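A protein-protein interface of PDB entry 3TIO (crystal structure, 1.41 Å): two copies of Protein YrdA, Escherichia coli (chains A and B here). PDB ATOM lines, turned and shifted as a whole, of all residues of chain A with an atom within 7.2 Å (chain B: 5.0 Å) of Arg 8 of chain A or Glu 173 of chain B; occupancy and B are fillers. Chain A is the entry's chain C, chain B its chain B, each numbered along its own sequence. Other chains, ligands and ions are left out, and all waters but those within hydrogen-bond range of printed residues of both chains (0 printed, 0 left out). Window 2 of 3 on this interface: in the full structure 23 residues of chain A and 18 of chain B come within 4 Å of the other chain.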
ATOM      1  N   PRO A   6       2.271  -2.902  30.091  1.00  0.00           N
ATOM      2  CA  PRO A   6       2.523  -1.508  29.734  1.00  0.00           C
ATOM      3  C   PRO A   6       1.297  -0.812  29.146  1.00  0.00           C
ATOM      4  O   PRO A   6       0.331  -1.459  28.739  1.00  0.00           O
ATOM      5  CB  PRO A   6       3.642  -1.628  28.708  1.00  0.00           C
ATOM      6  CG  PRO A   6       3.228  -2.855  27.952  1.00  0.00           C
ATOM      7  CD  PRO A   6       2.804  -3.815  29.060  1.00  0.00           C
ATOM      8  N   TYR A   7       1.348   0.514  29.141  1.00  0.00           N
ATOM      9  CA  TYR A   7       0.322   1.361  28.544  1.00  0.00           C
ATOM     10  C   TYR A   7       1.196   2.357  27.800  1.00  0.00           C
ATOM     11  O   TYR A   7       1.786   3.247  28.412  1.00  0.00           O
ATOM     12  CB  TYR A   7      -0.510   2.099  29.593  1.00  0.00           C
ATOM     13  CG  TYR A   7      -1.463   3.096  28.965  1.00  0.00           C
ATOM     14  CD1 TYR A   7      -2.505   2.668  28.145  1.00  0.00           C
ATOM     15  CD2 TYR A   7      -1.292   4.469  29.147  1.00  0.00           C
ATOM     16  CE1 TYR A   7      -3.354   3.580  27.519  1.00  0.00           C
ATOM     17  CE2 TYR A   7      -2.135   5.390  28.524  1.00  0.00           C
ATOM     18  CZ  TYR A   7      -3.163   4.937  27.710  1.00  0.00           C
ATOM     19  OH  TYR A   7      -3.989   5.839  27.079  1.00  0.00           O
ATOM     20  N   ARG A   8       1.291   2.201  26.483  1.00  0.00           N
ATOM     21  CA  ARG A   8       2.160   3.062  25.691  1.00  0.00           C
ATOM     22  C   ARG A   8       3.559   2.770  26.234  1.00  0.00           C
ATOM     23  O   ARG A   8       3.966   1.611  26.304  1.00  0.00           O
ATOM     24  CB  ARG A   8       1.811   4.541  25.892  1.00  0.00           C
ATOM     25  CG  ARG A   8       0.438   4.946  25.380  1.00  0.00           C
ATOM     26  CD  ARG A   8       0.157   6.408  25.699  1.00  0.00           C
ATOM     27  NE  ARG A   8      -1.162   6.837  25.245  1.00  0.00           N
ATOM     28  CZ  ARG A   8      -1.680   8.037  25.488  1.00  0.00           C
ATOM     29  NH1 ARG A   8      -0.989   8.931  26.184  1.00  0.00           N
ATOM     30  NH2 ARG A   8      -2.888   8.346  25.037  1.00  0.00           N
ATOM     31  N   ASP A   9       4.283   3.806  26.641  1.00  0.00           N
ATOM     32  CA  ASP A   9       5.623   3.612  27.181  1.00  0.00           C
ATOM     33  C   ASP A   9       5.629   3.710  28.705  1.00  0.00           C
ATOM     34  O   ASP A   9       6.661   3.985  29.318  1.00  0.00           O
ATOM     35  CB  ASP A   9       6.589   4.633  26.576  1.00  0.00           C
ATOM     36  CG  ASP A   9       6.238   6.059  26.942  1.00  0.00           C
ATOM     37  OD1 ASP A   9       5.038   6.397  26.934  1.00  0.00           O
ATOM     38  OD2 ASP A   9       7.166   6.845  27.228  1.00  0.00           O
ATOM     39  N   LEU A  10       4.463   3.483  29.307  1.00  0.00           N
ATOM     40  CA  LEU A  10       4.307   3.523  30.758  1.00  0.00           C
ATOM     41  C   LEU A  10       4.312   2.093  31.295  1.00  0.00           C
ATOM     42  O   LEU A  10       3.601   1.231  30.783  1.00  0.00           O
ATOM     43  CB  LEU A  10       2.987   4.200  31.129  1.00  0.00           C
ATOM     44  CG  LEU A  10       2.778   5.628  30.624  1.00  0.00           C
ATOM     45  CD1 LEU A  10       1.376   6.097  30.980  1.00  0.00           C
ATOM     46  CD2 LEU A  10       3.822   6.547  31.230  1.00  0.00           C
ATOM     47  N   PHE A  11       5.113   1.844  32.324  1.00  0.00           N
ATOM     48  CA  PHE A  11       5.207   0.505  32.899  1.00  0.00           C
ATOM     49  C   PHE A  11       5.398   0.596  34.409  1.00  0.00           C
ATOM     50  O   PHE A  11       5.981   1.553  34.912  1.00  0.00           O
ATOM     51  CB  PHE A  11       6.390  -0.242  32.271  1.00  0.00           C
ATOM     52  CG  PHE A  11       6.365  -1.724  32.500  1.00  0.00           C
ATOM     53  CD1 PHE A  11       5.522  -2.542  31.752  1.00  0.00           C
ATOM     54  CD2 PHE A  11       7.188  -2.309  33.460  1.00  0.00           C
ATOM     55  CE1 PHE A  11       5.499  -3.922  31.956  1.00  0.00           C
ATOM     56  CE2 PHE A  11       7.173  -3.688  33.672  1.00  0.00           C
ATOM     57  CZ  PHE A  11       6.326  -4.495  32.916  1.00  0.00           C
ATOM     58  N   GLY A  28       0.279  -0.011  33.228  1.00  0.00           N
ATOM     59  CA  GLY A  28       0.773   1.347  33.129  1.00  0.00           C
ATOM     60  C   GLY A  28       1.705   1.903  34.179  1.00  0.00           C
ATOM     61  O   GLY A  28       2.521   1.193  34.770  1.00  0.00           O
ATOM     62  N   ASP A  47      -3.231   4.465  33.477  1.00  0.00           N
ATOM     63  CA  ASP A  47      -3.046   4.829  32.080  1.00  0.00           C
ATOM     64  C   ASP A  47      -3.094   6.321  31.752  1.00  0.00           C
ATOM     65  O   ASP A  47      -2.164   6.839  31.126  1.00  0.00           O
ATOM     66  CB  ASP A  47      -4.012   4.045  31.162  1.00  0.00           C
ATOM     67  CG  ASP A  47      -5.377   3.783  31.784  1.00  0.00           C
ATOM     68  OD1 ASP A  47      -5.759   4.444  32.772  1.00  0.00           O
ATOM     69  OD2 ASP A  47      -6.085   2.901  31.245  1.00  0.00           O
ATOM     70  N   VAL A  48      -4.143   7.023  32.163  1.00  0.00           N
ATOM     71  CA  VAL A  48      -4.221   8.453  31.867  1.00  0.00           C
ATOM     72  C   VAL A  48      -3.453   9.298  32.881  1.00  0.00           C
ATOM     73  O   VAL A  48      -3.241  10.492  32.675  1.00  0.00           O
ATOM     74  CB  VAL A  48      -5.685   8.931  31.781  1.00  0.00           C
ATOM     75  CG1 VAL A  48      -6.352   8.319  30.557  1.00  0.00           C
ATOM     76  CG2 VAL A  48      -6.438   8.547  33.036  1.00  0.00           C
ATOM     77  N   LYS A  70     -10.093  11.671  32.073  1.00  0.00           N
ATOM     78  CA  LYS A  70      -9.997  12.993  31.468  1.00  0.00           C
ATOM     79  C   LYS A  70     -11.414  13.497  31.230  1.00  0.00           C
ATOM     80  O   LYS A  70     -12.260  12.762  30.722  1.00  0.00           O
ATOM     81  CB  LYS A  70      -9.256  12.919  30.132  1.00  0.00           C
ATOM     82  CG  LYS A  70      -7.843  12.378  30.226  1.00  0.00           C
ATOM     83  CD  LYS A  70      -7.179  12.351  28.860  1.00  0.00           C
ATOM     84  CE  LYS A  70      -5.777  11.769  28.940  1.00  0.00           C
ATOM     85  NZ  LYS A  70      -4.910  12.541  29.873  1.00  0.00           N
ATOM     86  N   LYS B 169     -12.127   5.625  22.370  1.00  0.00           N
ATOM     87  CA  LYS B 169     -10.757   5.997  22.037  1.00  0.00           C
ATOM     88  C   LYS B 169      -9.803   5.239  22.953  1.00  0.00           C
ATOM     89  O   LYS B 169      -8.743   4.786  22.528  1.00  0.00           O
ATOM     90  CB  LYS B 169     -10.546   7.500  22.225  1.00  0.00           C
ATOM     91  CG  LYS B 169     -11.324   8.376  21.260  1.00  0.00           C
ATOM     92  CD  LYS B 169     -11.103   9.852  21.567  1.00  0.00           C
ATOM     93  CE  LYS B 169      -9.630  10.227  21.487  1.00  0.00           C
ATOM     94  NZ  LYS B 169      -9.399  11.656  21.841  1.00  0.00           N
ATOM     95  N   TRP B 170     -10.198   5.106  24.218  1.00  0.00           N
ATOM     96  CA  TRP B 170      -9.404   4.408  25.224  1.00  0.00           C
ATOM     97  C   TRP B 170      -9.208   2.950  24.807  1.00  0.00           C
ATOM     98  O   TRP B 170      -8.105   2.409  24.887  1.00  0.00           O
ATOM     99  CB  TRP B 170     -10.129   4.456  26.570  1.00  0.00           C
ATOM    100  CG  TRP B 170      -9.243   4.657  27.754  1.00  0.00           C
ATOM    101  CD1 TRP B 170      -7.942   4.265  27.889  1.00  0.00           C
ATOM    102  CD2 TRP B 170      -9.612   5.261  28.998  1.00  0.00           C
ATOM    103  NE1 TRP B 170      -7.478   4.589  29.143  1.00  0.00           N
ATOM    104  CE2 TRP B 170      -8.484   5.200  29.844  1.00  0.00           C
ATOM    105  CE3 TRP B 170     -10.790   5.847  29.482  1.00  0.00           C
ATOM    106  CZ2 TRP B 170      -8.497   5.703  31.149  1.00  0.00           C
ATOM    107  CZ3 TRP B 170     -10.803   6.348  30.782  1.00  0.00           C
ATOM    108  CH2 TRP B 170      -9.663   6.271  31.598  1.00  0.00           C
ATOM    109  N   LYS B 171     -10.301   2.324  24.379  1.00  0.00           N
ATOM    110  CA  LYS B 171     -10.295   0.935  23.926  1.00  0.00           C
ATOM    111  C   LYS B 171      -9.346   0.764  22.746  1.00  0.00           C
ATOM    112  O   LYS B 171      -8.554  -0.181  22.697  1.00  0.00           O
ATOM    113  CB  LYS B 171     -11.711   0.527  23.496  1.00  0.00           C
ATOM    114  CG  LYS B 171     -11.758  -0.568  22.433  1.00  0.00           C
ATOM    115  CD  LYS B 171     -13.151  -0.698  21.837  1.00  0.00           C
ATOM    116  CE  LYS B 171     -13.478   0.451  20.883  1.00  0.00           C
ATOM    117  NZ  LYS B 171     -12.907   0.245  19.519  1.00  0.00           N
ATOM    118  N   ASP B 172      -9.436   1.679  21.789  1.00  0.00           N
ATOM    119  CA  ASP B 172      -8.585   1.610  20.611  1.00  0.00           C
ATOM    120  C   ASP B 172      -7.121   1.783  20.970  1.00  0.00           C
ATOM    121  O   ASP B 172      -6.245   1.205  20.327  1.00  0.00           O
ATOM    122  CB  ASP B 172      -9.019   2.658  19.585  1.00  0.00           C
ATOM    123  CG  ASP B 172     -10.351   2.320  18.952  1.00  0.00           C
ATOM    124  OD1 ASP B 172     -10.586   1.120  18.691  1.00  0.00           O
ATOM    125  OD2 ASP B 172     -11.156   3.240  18.706  1.00  0.00           O
ATOM    126  N   GLU B 173      -6.863   2.567  22.010  1.00  0.00           N
ATOM    127  CA  GLU B 173      -5.504   2.800  22.477  1.00  0.00           C
ATOM    128  C   GLU B 173      -4.875   1.459  22.860  1.00  0.00           C
ATOM    129  O   GLU B 173      -3.737   1.174  22.496  1.00  0.00           O
ATOM    130  CB  GLU B 173      -5.523   3.729  23.694  1.00  0.00           C
ATOM    131  CG  GLU B 173      -4.153   4.176  24.177  1.00  0.00           C
ATOM    132  CD  GLU B 173      -3.607   5.352  23.388  1.00  0.00           C
ATOM    133  OE1 GLU B 173      -4.249   6.425  23.398  1.00  0.00           O
ATOM    134  OE2 GLU B 173      -2.535   5.208  22.762  1.00  0.00           O
ATOM    135  N   TYR B 174      -5.622   0.636  23.593  1.00  0.00           N
ATOM    136  CA  TYR B 174      -5.116  -0.668  24.015  1.00  0.00           C
ATOM    137  C   TYR B 174      -5.023  -1.676  22.881  1.00  0.00           C
ATOM    138  O   TYR B 174      -4.093  -2.480  22.837  1.00  0.00           O
ATOM    139  CB  TYR B 174      -5.976  -1.250  25.141  1.00  0.00           C
ATOM    140  CG  TYR B 174      -5.615  -0.713  26.503  1.00  0.00           C
ATOM    141  CD1 TYR B 174      -6.113   0.512  26.945  1.00  0.00           C
ATOM    142  CD2 TYR B 174      -4.741  -1.411  27.334  1.00  0.00           C
ATOM    143  CE1 TYR B 174      -5.747   1.029  28.184  1.00  0.00           C
ATOM    144  CE2 TYR B 174      -4.367  -0.901  28.573  1.00  0.00           C
ATOM    145  CZ  TYR B 174      -4.874   0.319  28.992  1.00  0.00           C
ATOM    146  OH  TYR B 174      -4.505   0.825  30.216  1.00  0.00           O
ATOM    147  N   LEU B 175      -5.990  -1.641  21.970  1.00  0.00           N
ATOM    148  CA  LEU B 175      -5.980  -2.559  20.840  1.00  0.00           C
ATOM    149  C   LEU B 175      -4.754  -2.311  19.969  1.00  0.00           C
ATOM    150  O   LEU B 175      -4.128  -3.254  19.486  1.00  0.00           O
ATOM    151  CB  LEU B 175      -7.252  -2.396  20.004  1.00  0.00           C
ATOM    152  CG  LEU B 175      -8.546  -2.960  20.593  1.00  0.00           C
ATOM    153  CD1 LEU B 175      -9.718  -2.604  19.692  1.00  0.00           C
ATOM    154  CD2 LEU B 175      -8.426  -4.474  20.742  1.00  0.00           C
ATOM    155  N   ASP B 176      -4.408  -1.041  19.781  1.00  0.00           N
ATOM    156  CA  ASP B 176      -3.256  -0.687  18.961  1.00  0.00           C
ATOM    157  C   ASP B 176      -1.947  -1.161  19.580  1.00  0.00           C
ATOM    158  O   ASP B 176      -0.880  -1.001  18.988  1.00  0.00           O
ATOM    159  CB  ASP B 176      -3.198   0.827  18.733  1.00  0.00           C
ATOM    160  CG  ASP B 176      -4.371   1.339  17.921  1.00  0.00           C
ATOM    161  OD1 ASP B 176      -4.750   0.676  16.932  1.00  0.00           O
ATOM    162  OD2 ASP B 176      -4.908   2.415  18.262  1.00  0.00           O
ATOM    163  N   GLN B 177      -2.031  -1.742  20.772  1.00  0.00           N
ATOM    164  CA  GLN B 177      -0.847  -2.249  21.459  1.00  0.00           C
ATOM    165  C   GLN B 177      -0.826  -3.774  21.409  1.00  0.00           C
ATOM    166  O   GLN B 177      -0.797  -4.401  22.489  1.00  0.00           O
ATOM    167  CB  GLN B 177      -0.835  -1.785  22.918  1.00  0.00           C
ATOM    168  CG  GLN B 177      -0.864  -0.277  23.102  1.00  0.00           C
ATOM    169  CD  GLN B 177      -0.685   0.136  24.553  1.00  0.00           C
ATOM    170  OE1 GLN B 177      -0.777   1.316  24.890  1.00  0.00           O
ATOM    171  NE2 GLN B 177      -0.421  -0.838  25.420  1.00  0.00           N
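Among the printed residues, pairs that only touch across the chains: Tyr 7 of chain A with Glu 173 of chain B (3.3 Å), Tyr 7 of chain A with Tyr 174 of chain B (3.4 Å), Tyr 7 of chain A with Gln 177 of chain B (3.7 Å) and Val 48 of chain A with Trp 170 of chain B (3.4 Å).
Of the 9 printed residues of chain B, 4 touch a printed residue of chain A.
Printed residues of chain A that touch a printed residue of chain B: Pro 6, Tyr 7, Arg 8, Asp 47 and Val 48.
Among the printed residues, 9 pairs touch across the chains.
Among the printed residues, Asp or Glu carboxylates within 4 Å of a Lys or Arg side-chain nitrogen of the other chain: Arg 8 of chain A with Glu 173 of chain B (2.9 Å).
The indole nitrogen (NE1) of Trp 170 of chain B sits at hydrogen-bond distance from the side-chain carboxylate (OD2) of Asp 47 of chain A (3.0 Å).
NE2 of Gln 177 of chain B is in hydrogen-bond range of O of Pro 6 of chain A.
N of Arg 8 of chain A sits at hydrogen-bond distance from OE1 of Gln 177 of chain B, at 2.8 Å.
The side-chain hydroxyl (OH) of Tyr 174 of chain B is in hydrogen-bond range of the side-chain carboxylate (OD2) of Asp 47 of chain A, at 2.8 Å.
The side-chain carboxylate of Glu 173 of chain B lies within salt-bridge range of the guanidinium group of Arg 8 of chain A, at 2.9 Å.
OH of Tyr 7 of chain A lies within hydrogen-bond range of NH2 of Arg 8 of chain A, 3.4 Å away.
No position is printed for both chains.
Of the printed residues of chain B, Pro 6 of chain A touches Gln 177.
Printed residues of chain B within 4 Å of Tyr 7 of chain A: Glu 173, Tyr 174 and Gln 177.
Of chain B, only Glu 173 and Gln 177 come within 4 Å of Arg 8 of chain A.
Of the printed residues of chain B, Asp 47 of chain A touches Trp 170 (3.0 Å) and Tyr 174 (2.8 Å).
Of the printed residues of chain A, Trp 170 of chain B touches Asp 47 and Val 48.
Lys 171 of chain B touches none of the printed residues of chain A.
Asp 172 of chain B touches none of the printed residues of chain A.
Glu 173 of chain B touches just these residues of chain A: Tyr 7 and Arg 8.
The nearest printed residue of chain B that does not touch Pro 6 of chain A is Tyr 174 of chain B (4.7 Å).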
